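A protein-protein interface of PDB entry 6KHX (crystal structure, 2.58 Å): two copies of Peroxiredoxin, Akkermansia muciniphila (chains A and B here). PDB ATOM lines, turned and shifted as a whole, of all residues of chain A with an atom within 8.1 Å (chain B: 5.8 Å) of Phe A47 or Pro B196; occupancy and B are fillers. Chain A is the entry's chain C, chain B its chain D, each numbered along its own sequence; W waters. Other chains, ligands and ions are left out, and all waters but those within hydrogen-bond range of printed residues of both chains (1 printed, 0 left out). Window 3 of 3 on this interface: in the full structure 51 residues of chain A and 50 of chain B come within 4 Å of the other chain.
O of Phe A47 lies close to SD of Met B194.
The side-chain hydroxyl (OG) of Ser B197 lies within hydrogen-bond range of the backbone NH (N) of Gly B200 (3.0 Å). N of Val B182 sits at hydrogen-bond distance from O of Met B194. OG1 of Thr A46 is in hydrogen-bond range of O of Lys A43 (2.7 Å). The side-chain hydroxyl (OG1) of Thr A46 is in hydrogen-bond range of the side-chain sulfur (SG) of Cys A49, at 3.3 Å. The side-chain hydroxyl of Thr A51 is in hydrogen-bond range of the backbone carbonyl oxygen of Val A48 (2.7 Å).
Among the printed residues, pairs that only touch across the chains: Phe A47 with Ser B197, Thr A46 with Val B201, Phe A47 with Pro B196, Thr A51 with Met B194, Pro A158 with Phe B176, Val A48 with Val B182, Pro A158 with Val B182, Pro A50 with Val B201, Phe A47 with His B198 and Phe A47 with Val B201.
Pro A42 touches none of the printed residues of chain B. Lys A43 touches none of the printed residues of chain B. Printed residues of chain B within 4 Å of Thr A46: Val B201 (3.4 Å). Phe A47 touches five residues of chain B. Of the printed residues of chain B, Pro A50 touches Val B201. Of the printed residues of chain A, Val B182 touches Val A48 (3.6 Å) and Pro A158 (3.6 Å). Printed residues of chain A within 4 Å of Met B194: Phe A47 (3.5 Å) and Thr A51 (3.4 Å). Pro B196 touches just one residue of chain A: Phe A47 (3.4 Å). Of the printed residues of chain A, His B198 touches Phe A47. The nearest residue of chain A that does not touch Pro B196 is Val A48 (7.0 Å). The nearest printed residue of chain B that does not touch Pro A158 is Glu B181 (5.2 Å).
Hydrophobic or aromatic side chains of chain B that line the printed part of chain A: Phe B176, Val B182, Met B194, Pro B196 and Val B201. Among the printed residues, 11 pairs touch across the chains.
No position is printed for both chains.
Water W1 lies within hydrogen-bond range of ND1 of His B198 (2.5 Å) and O of Phe A45 (3.1 Å).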
ATOM      1  N   PRO A  42      10.408 -11.421 -22.386  1.00  0.00           N
ATOM      2  CA  PRO A  42      10.924 -11.534 -21.008  1.00  0.00           C
ATOM      3  C   PRO A  42      11.262 -12.934 -20.501  1.00  0.00           C
ATOM      4  O   PRO A  42      12.333 -13.114 -19.911  1.00  0.00           O
ATOM      5  CB  PRO A  42       9.804 -10.908 -20.164  1.00  0.00           C
ATOM      6  CG  PRO A  42       8.598 -10.991 -21.003  1.00  0.00           C
ATOM      7  CD  PRO A  42       9.055 -10.843 -22.414  1.00  0.00           C
ATOM      8  N   LYS A  43      10.379 -13.922 -20.661  1.00  0.00           N
ATOM      9  CA  LYS A  43      10.574 -15.198 -19.977  1.00  0.00           C
ATOM     10  C   LYS A  43      10.112 -16.373 -20.827  1.00  0.00           C
ATOM     11  O   LYS A  43       9.029 -16.332 -21.419  1.00  0.00           O
ATOM     12  CB  LYS A  43       9.817 -15.226 -18.645  1.00  0.00           C
ATOM     13  CG  LYS A  43      10.564 -14.641 -17.480  1.00  0.00           C
ATOM     14  CD  LYS A  43       9.711 -14.664 -16.234  1.00  0.00           C
ATOM     15  CE  LYS A  43      10.245 -13.701 -15.204  1.00  0.00           C
ATOM     16  NZ  LYS A  43       9.311 -13.572 -14.061  1.00  0.00           N
ATOM     17  N   ASP A  44      10.936 -17.418 -20.881  1.00  0.00           N
ATOM     18  CA  ASP A  44      10.481 -18.696 -21.409  1.00  0.00           C
ATOM     19  C   ASP A  44       9.362 -19.279 -20.544  1.00  0.00           C
ATOM     20  O   ASP A  44       9.274 -19.026 -19.336  1.00  0.00           O
ATOM     21  CB  ASP A  44      11.636 -19.698 -21.490  1.00  0.00           C
ATOM     22  CG  ASP A  44      12.588 -19.417 -22.638  1.00  0.00           C
ATOM     23  OD1 ASP A  44      12.361 -18.455 -23.407  1.00  0.00           O
ATOM     24  OD2 ASP A  44      13.554 -20.195 -22.786  1.00  0.00           O
ATOM     25  N   PHE A  45       8.504 -20.079 -21.183  1.00  0.00           N
ATOM     26  CA  PHE A  45       7.431 -20.807 -20.514  1.00  0.00           C
ATOM     27  C   PHE A  45       6.375 -19.881 -19.914  1.00  0.00           C
ATOM     28  O   PHE A  45       5.762 -20.206 -18.895  1.00  0.00           O
ATOM     29  CB  PHE A  45       7.976 -21.740 -19.429  1.00  0.00           C
ATOM     30  CG  PHE A  45       8.972 -22.746 -19.928  1.00  0.00           C
ATOM     31  CD1 PHE A  45       8.551 -23.871 -20.628  1.00  0.00           C
ATOM     32  CD2 PHE A  45      10.322 -22.602 -19.650  1.00  0.00           C
ATOM     33  CE1 PHE A  45       9.461 -24.815 -21.072  1.00  0.00           C
ATOM     34  CE2 PHE A  45      11.239 -23.547 -20.089  1.00  0.00           C
ATOM     35  CZ  PHE A  45      10.807 -24.658 -20.800  1.00  0.00           C
ATOM     36  N   THR A  46       6.142 -18.721 -20.521  1.00  0.00           N
ATOM     37  CA  THR A  46       5.076 -17.862 -20.029  1.00  0.00           C
ATOM     38  C   THR A  46       3.930 -17.788 -21.033  1.00  0.00           C
ATOM     39  O   THR A  46       3.577 -18.798 -21.651  1.00  0.00           O
ATOM     40  CB  THR A  46       5.611 -16.472 -19.688  1.00  0.00           C
ATOM     41  OG1 THR A  46       6.420 -15.994 -20.765  1.00  0.00           O
ATOM     42  CG2 THR A  46       6.451 -16.539 -18.426  1.00  0.00           C
ATOM     43  N   PHE A  47       3.358 -16.597 -21.219  1.00  0.00           N
ATOM     44  CA  PHE A  47       2.018 -16.465 -21.779  1.00  0.00           C
ATOM     45  C   PHE A  47       2.014 -15.760 -23.134  1.00  0.00           C
ATOM     46  O   PHE A  47       1.729 -16.401 -24.147  1.00  0.00           O
ATOM     47  CB  PHE A  47       1.128 -15.753 -20.754  1.00  0.00           C
ATOM     48  CG  PHE A  47       1.386 -16.195 -19.322  1.00  0.00           C
ATOM     49  CD1 PHE A  47       1.456 -17.544 -18.992  1.00  0.00           C
ATOM     50  CD2 PHE A  47       1.574 -15.264 -18.315  1.00  0.00           C
ATOM     51  CE1 PHE A  47       1.713 -17.948 -17.694  1.00  0.00           C
ATOM     52  CE2 PHE A  47       1.817 -15.665 -17.011  1.00  0.00           C
ATOM     53  CZ  PHE A  47       1.886 -17.008 -16.703  1.00  0.00           C
ATOM     54  N   VAL A  48       2.320 -14.460 -23.190  1.00  0.00           N
ATOM     55  CA  VAL A  48       2.331 -13.759 -24.476  1.00  0.00           C
ATOM     56  C   VAL A  48       3.505 -14.223 -25.336  1.00  0.00           C
ATOM     57  O   VAL A  48       3.399 -14.314 -26.572  1.00  0.00           O
ATOM     58  CB  VAL A  48       2.379 -12.236 -24.254  1.00  0.00           C
ATOM     59  CG1 VAL A  48       2.394 -11.496 -25.586  1.00  0.00           C
ATOM     60  CG2 VAL A  48       1.220 -11.775 -23.405  1.00  0.00           C
ATOM     61  N   CYS A  49       4.636 -14.520 -24.696  1.00  0.00           N
ATOM     62  CA  CYS A  49       5.860 -14.845 -25.427  1.00  0.00           C
ATOM     63  C   CYS A  49       5.703 -16.026 -26.377  1.00  0.00           C
ATOM     64  O   CYS A  49       6.148 -15.917 -27.535  1.00  0.00           O
ATOM     65  CB  CYS A  49       7.003 -15.059 -24.425  1.00  0.00           C
ATOM     66  SG  CYS A  49       7.071 -13.787 -23.106  1.00  0.00           S
ATOM     67  N   PRO A  50       5.114 -17.160 -25.982  1.00  0.00           N
ATOM     68  CA  PRO A  50       4.934 -18.238 -26.968  1.00  0.00           C
ATOM     69  C   PRO A  50       4.058 -17.832 -28.135  1.00  0.00           C
ATOM     70  O   PRO A  50       4.321 -18.262 -29.261  1.00  0.00           O
ATOM     71  CB  PRO A  50       4.309 -19.374 -26.147  1.00  0.00           C
ATOM     72  CG  PRO A  50       3.733 -18.708 -24.948  1.00  0.00           C
ATOM     73  CD  PRO A  50       4.656 -17.577 -24.643  1.00  0.00           C
ATOM     74  N   THR A  51       3.028 -17.012 -27.914  1.00  0.00           N
ATOM     75  CA  THR A  51       2.199 -16.603 -29.044  1.00  0.00           C
ATOM     76  C   THR A  51       3.000 -15.757 -30.019  1.00  0.00           C
ATOM     77  O   THR A  51       2.887 -15.934 -31.237  1.00  0.00           O
ATOM     78  CB  THR A  51       0.955 -15.839 -28.576  1.00  0.00           C
ATOM     79  OG1 THR A  51       1.280 -14.467 -28.315  1.00  0.00           O
ATOM     80  CG2 THR A  51       0.410 -16.468 -27.317  1.00  0.00           C
ATOM     81  N   GLU A  52       3.845 -14.856 -29.508  1.00  0.00           N
ATOM     82  CA  GLU A  52       4.658 -14.049 -30.414  1.00  0.00           C
ATOM     83  C   GLU A  52       5.660 -14.912 -31.176  1.00  0.00           C
ATOM     84  O   GLU A  52       5.826 -14.754 -32.396  1.00  0.00           O
ATOM     85  CB  GLU A  52       5.368 -12.942 -29.638  1.00  0.00           C
ATOM     86  CG  GLU A  52       4.418 -12.006 -28.926  1.00  0.00           C
ATOM     87  CD  GLU A  52       5.120 -10.834 -28.280  1.00  0.00           C
ATOM     88  OE1 GLU A  52       4.883  -9.684 -28.709  1.00  0.00           O
ATOM     89  OE2 GLU A  52       5.898 -11.059 -27.330  1.00  0.00           O
ATOM     90  N   LEU A  53       6.323 -15.841 -30.478  1.00  0.00           N
ATOM     91  CA  LEU A  53       7.312 -16.690 -31.139  1.00  0.00           C
ATOM     92  C   LEU A  53       6.663 -17.596 -32.190  1.00  0.00           C
ATOM     93  O   LEU A  53       7.168 -17.723 -33.318  1.00  0.00           O
ATOM     94  CB  LEU A  53       8.074 -17.509 -30.093  1.00  0.00           C
ATOM     95  CG  LEU A  53       9.112 -16.723 -29.279  1.00  0.00           C
ATOM     96  CD1 LEU A  53       9.189 -17.214 -27.839  1.00  0.00           C
ATOM     97  CD2 LEU A  53      10.483 -16.776 -29.932  1.00  0.00           C
ATOM     98  N   ILE A  54       5.530 -18.218 -31.846  1.00  0.00           N
ATOM     99  CA  ILE A  54       4.829 -19.082 -32.788  1.00  0.00           C
ATOM    100  C   ILE A  54       4.331 -18.279 -33.978  1.00  0.00           C
ATOM    101  O   ILE A  54       4.442 -18.719 -35.127  1.00  0.00           O
ATOM    102  CB  ILE A  54       3.679 -19.824 -32.085  1.00  0.00           C
ATOM    103  CG1 ILE A  54       4.233 -20.870 -31.115  1.00  0.00           C
ATOM    104  CG2 ILE A  54       2.748 -20.465 -33.110  1.00  0.00           C
ATOM    105  CD1 ILE A  54       3.203 -21.405 -30.134  1.00  0.00           C
ATOM    106  N   TRP A  84      12.004 -25.559 -24.407  1.00  0.00           N
ATOM    107  CA  TRP A  84      10.743 -24.943 -24.800  1.00  0.00           C
ATOM    108  C   TRP A  84      10.361 -25.320 -26.228  1.00  0.00           C
ATOM    109  O   TRP A  84       9.177 -25.523 -26.523  1.00  0.00           O
ATOM    110  CB  TRP A  84      10.835 -23.426 -24.641  1.00  0.00           C
ATOM    111  CG  TRP A  84       9.527 -22.772 -24.357  1.00  0.00           C
ATOM    112  CD1 TRP A  84       8.381 -23.380 -23.936  1.00  0.00           C
ATOM    113  CD2 TRP A  84       9.224 -21.377 -24.470  1.00  0.00           C
ATOM    114  NE1 TRP A  84       7.382 -22.448 -23.777  1.00  0.00           N
ATOM    115  CE2 TRP A  84       7.873 -21.212 -24.102  1.00  0.00           C
ATOM    116  CE3 TRP A  84       9.964 -20.251 -24.847  1.00  0.00           C
ATOM    117  CZ2 TRP A  84       7.248 -19.966 -24.098  1.00  0.00           C
ATOM    118  CZ3 TRP A  84       9.341 -19.015 -24.843  1.00  0.00           C
ATOM    119  CH2 TRP A  84       7.997 -18.882 -24.469  1.00  0.00           C
ATOM    120  N   GLY A  92       1.662 -25.078 -23.877  1.00  0.00           N
ATOM    121  CA  GLY A  92       2.375 -23.828 -23.731  1.00  0.00           C
ATOM    122  C   GLY A  92       3.740 -23.773 -24.378  1.00  0.00           C
ATOM    123  O   GLY A  92       4.442 -22.770 -24.207  1.00  0.00           O
ATOM    124  N   ILE A  94       6.716 -24.040 -27.608  1.00  0.00           N
ATOM    125  CA  ILE A  94       6.947 -23.343 -28.869  1.00  0.00           C
ATOM    126  C   ILE A  94       7.557 -24.311 -29.873  1.00  0.00           C
ATOM    127  O   ILE A  94       8.440 -23.942 -30.656  1.00  0.00           O
ATOM    128  CB  ILE A  94       7.846 -22.109 -28.672  1.00  0.00           C
ATOM    129  CG1 ILE A  94       9.168 -22.509 -28.011  1.00  0.00           C
ATOM    130  CG2 ILE A  94       7.130 -21.062 -27.839  1.00  0.00           C
ATOM    131  CD1 ILE A  94      10.234 -21.464 -28.135  1.00  0.00           C
ATOM    132  N   ARG A 138       9.249  -6.251 -24.164  1.00  0.00           N
ATOM    133  CA  ARG A 138       8.881  -6.692 -25.509  1.00  0.00           C
ATOM    134  C   ARG A 138       9.449  -5.704 -26.522  1.00  0.00           C
ATOM    135  O   ARG A 138       8.785  -4.776 -26.990  1.00  0.00           O
ATOM    136  CB  ARG A 138       7.374  -6.853 -25.635  1.00  0.00           C
ATOM    137  CG  ARG A 138       6.868  -7.939 -24.711  1.00  0.00           C
ATOM    138  CD  ARG A 138       5.426  -8.351 -24.946  1.00  0.00           C
ATOM    139  NE  ARG A 138       4.998  -9.152 -23.809  1.00  0.00           N
ATOM    140  CZ  ARG A 138       5.344 -10.420 -23.632  1.00  0.00           C
ATOM    141  NH1 ARG A 138       6.100 -11.035 -24.532  1.00  0.00           N
ATOM    142  NH2 ARG A 138       4.937 -11.073 -22.555  1.00  0.00           N
ATOM    143  N   PHE A 157       4.916  -5.629 -20.643  1.00  0.00           N
ATOM    144  CA  PHE A 157       4.795  -7.087 -20.564  1.00  0.00           C
ATOM    145  C   PHE A 157       3.477  -7.659 -21.086  1.00  0.00           C
ATOM    146  O   PHE A 157       3.524  -8.645 -21.838  1.00  0.00           O
ATOM    147  CB  PHE A 157       5.057  -7.514 -19.113  1.00  0.00           C
ATOM    148  CG  PHE A 157       6.475  -7.287 -18.667  1.00  0.00           C
ATOM    149  CD1 PHE A 157       7.537  -7.650 -19.481  1.00  0.00           C
ATOM    150  CD2 PHE A 157       6.749  -6.692 -17.449  1.00  0.00           C
ATOM    151  CE1 PHE A 157       8.848  -7.437 -19.075  1.00  0.00           C
ATOM    152  CE2 PHE A 157       8.054  -6.474 -17.041  1.00  0.00           C
ATOM    153  CZ  PHE A 157       9.105  -6.847 -17.854  1.00  0.00           C
ATOM    154  N   PRO A 158       2.295  -7.140 -20.735  1.00  0.00           N
ATOM    155  CA  PRO A 158       1.053  -7.790 -21.181  1.00  0.00           C
ATOM    156  C   PRO A 158       0.585  -7.417 -22.580  1.00  0.00           C
ATOM    157  O   PRO A 158      -0.501  -7.859 -22.974  1.00  0.00           O
ATOM    158  CB  PRO A 158       0.023  -7.336 -20.131  1.00  0.00           C
ATOM    159  CG  PRO A 158       0.588  -6.123 -19.488  1.00  0.00           C
ATOM    160  CD  PRO A 158       2.017  -5.943 -19.921  1.00  0.00           C
ATOM    161  N   PHE B 176      -6.228  -5.116 -21.015  1.00  0.00           N
ATOM    162  CA  PHE B 176      -5.513  -5.661 -19.865  1.00  0.00           C
ATOM    163  C   PHE B 176      -5.935  -4.969 -18.576  1.00  0.00           C
ATOM    164  O   PHE B 176      -6.015  -5.611 -17.521  1.00  0.00           O
ATOM    165  CB  PHE B 176      -4.003  -5.550 -20.052  1.00  0.00           C
ATOM    166  CG  PHE B 176      -3.223  -5.911 -18.822  1.00  0.00           C
ATOM    167  CD1 PHE B 176      -3.075  -7.237 -18.446  1.00  0.00           C
ATOM    168  CD2 PHE B 176      -2.649  -4.926 -18.032  1.00  0.00           C
ATOM    169  CE1 PHE B 176      -2.363  -7.577 -17.311  1.00  0.00           C
ATOM    170  CE2 PHE B 176      -1.934  -5.256 -16.897  1.00  0.00           C
ATOM    171  CZ  PHE B 176      -1.792  -6.581 -16.535  1.00  0.00           C
ATOM    172  N   GLY B 180      -7.701  -8.005 -16.839  1.00  0.00           N
ATOM    173  CA  GLY B 180      -6.549  -8.741 -16.345  1.00  0.00           C
ATOM    174  C   GLY B 180      -6.020  -9.789 -17.300  1.00  0.00           C
ATOM    175  O   GLY B 180      -5.172 -10.599 -16.911  1.00  0.00           O
ATOM    176  N   GLU B 181      -6.524  -9.816 -18.527  1.00  0.00           N
ATOM    177  CA  GLU B 181      -6.049 -10.717 -19.560  1.00  0.00           C
ATOM    178  C   GLU B 181      -4.926 -10.058 -20.347  1.00  0.00           C
ATOM    179  O   GLU B 181      -5.015  -8.881 -20.707  1.00  0.00           O
ATOM    180  CB  GLU B 181      -7.189 -11.088 -20.510  1.00  0.00           C
ATOM    181  CG  GLU B 181      -8.320 -11.871 -19.874  1.00  0.00           C
ATOM    182  CD  GLU B 181      -9.471 -12.097 -20.834  1.00  0.00           C
ATOM    183  OE1 GLU B 181      -9.590 -11.334 -21.819  1.00  0.00           O
ATOM    184  OE2 GLU B 181     -10.247 -13.047 -20.612  1.00  0.00           O
ATOM    185  N   VAL B 182      -3.864 -10.817 -20.600  1.00  0.00           N
ATOM    186  CA  VAL B 182      -2.774 -10.333 -21.440  1.00  0.00           C
ATOM    187  C   VAL B 182      -3.152 -10.540 -22.901  1.00  0.00           C
ATOM    188  O   VAL B 182      -3.878 -11.478 -23.248  1.00  0.00           O
ATOM    189  CB  VAL B 182      -1.451 -11.037 -21.076  1.00  0.00           C
ATOM    190  CG1 VAL B 182      -1.078 -10.723 -19.640  1.00  0.00           C
ATOM    191  CG2 VAL B 182      -1.560 -12.544 -21.272  1.00  0.00           C
ATOM    192  N   MET B 194      -6.041 -13.780 -23.372  1.00  0.00           N
ATOM    193  CA  MET B 194      -5.436 -14.910 -22.681  1.00  0.00           C
ATOM    194  C   MET B 194      -5.357 -14.628 -21.188  1.00  0.00           C
ATOM    195  O   MET B 194      -5.060 -13.505 -20.773  1.00  0.00           O
ATOM    196  CB  MET B 194      -4.033 -15.208 -23.219  1.00  0.00           C
ATOM    197  CG  MET B 194      -3.305 -16.300 -22.443  1.00  0.00           C
ATOM    198  SD  MET B 194      -1.601 -16.487 -22.973  1.00  0.00           S
ATOM    199  CE  MET B 194      -1.809 -16.246 -24.722  1.00  0.00           C
ATOM    200  N   THR B 195      -5.625 -15.650 -20.391  1.00  0.00           N
ATOM    201  CA  THR B 195      -5.412 -15.554 -18.954  1.00  0.00           C
ATOM    202  C   THR B 195      -3.938 -15.793 -18.635  1.00  0.00           C
ATOM    203  O   THR B 195      -3.389 -16.835 -19.010  1.00  0.00           O
ATOM    204  CB  THR B 195      -6.292 -16.568 -18.221  1.00  0.00           C
ATOM    205  OG1 THR B 195      -7.671 -16.262 -18.462  1.00  0.00           O
ATOM    206  CG2 THR B 195      -6.017 -16.552 -16.725  1.00  0.00           C
ATOM    207  N   PRO B 196      -3.276 -14.874 -17.927  1.00  0.00           N
ATOM    208  CA  PRO B 196      -1.847 -15.063 -17.643  1.00  0.00           C
ATOM    209  C   PRO B 196      -1.572 -16.134 -16.604  1.00  0.00           C
ATOM    210  O   PRO B 196      -1.220 -15.832 -15.458  1.00  0.00           O
ATOM    211  CB  PRO B 196      -1.402 -13.678 -17.151  1.00  0.00           C
ATOM    212  CG  PRO B 196      -2.638 -13.045 -16.606  1.00  0.00           C
ATOM    213  CD  PRO B 196      -3.768 -13.559 -17.472  1.00  0.00           C
ATOM    214  N   SER B 197      -1.693 -17.395 -17.010  1.00  0.00           N
ATOM    215  CA  SER B 197      -1.376 -18.519 -16.139  1.00  0.00           C
ATOM    216  C   SER B 197      -0.966 -19.698 -17.006  1.00  0.00           C
ATOM    217  O   SER B 197      -1.176 -19.708 -18.226  1.00  0.00           O
ATOM    218  CB  SER B 197      -2.556 -18.923 -15.248  1.00  0.00           C
ATOM    219  OG  SER B 197      -3.598 -19.490 -16.026  1.00  0.00           O
ATOM    220  N   HIS B 198      -0.387 -20.705 -16.352  1.00  0.00           N
ATOM    221  CA  HIS B 198      -0.037 -21.936 -17.049  1.00  0.00           C
ATOM    222  C   HIS B 198      -1.242 -22.476 -17.816  1.00  0.00           C
ATOM    223  O   HIS B 198      -1.171 -22.737 -19.028  1.00  0.00           O
ATOM    224  CB  HIS B 198       0.468 -22.970 -16.043  1.00  0.00           C
ATOM    225  CG  HIS B 198       1.571 -22.474 -15.154  1.00  0.00           C
ATOM    226  ND1 HIS B 198       2.756 -21.966 -15.644  1.00  0.00           N
ATOM    227  CD2 HIS B 198       1.685 -22.455 -13.806  1.00  0.00           C
ATOM    228  CE1 HIS B 198       3.541 -21.633 -14.636  1.00  0.00           C
ATOM    229  NE2 HIS B 198       2.916 -21.922 -13.508  1.00  0.00           N
ATOM    230  N   GLY B 200      -3.898 -20.841 -18.641  1.00  0.00           N
ATOM    231  CA  GLY B 200      -4.338 -19.880 -19.639  1.00  0.00           C
ATOM    232  C   GLY B 200      -3.600 -20.014 -20.955  1.00  0.00           C
ATOM    233  O   GLY B 200      -4.211 -20.036 -22.028  1.00  0.00           O
ATOM    234  N   VAL B 201      -2.270 -20.109 -20.896  1.00  0.00           N
ATOM    235  CA  VAL B 201      -1.497 -20.203 -22.131  1.00  0.00           C
ATOM    236  C   VAL B 201      -1.694 -21.567 -22.783  1.00  0.00           C
ATOM    237  O   VAL B 201      -1.828 -21.665 -24.011  1.00  0.00           O
ATOM    238  CB  VAL B 201      -0.008 -19.888 -21.868  1.00  0.00           C
ATOM    239  CG1 VAL B 201       0.594 -20.843 -20.849  1.00  0.00           C
ATOM    240  CG2 VAL B 201       0.779 -19.934 -23.160  1.00  0.00           C
HETATM  241  O   HOH W   1       3.005 -21.199 -18.023  1.00  0.00           O
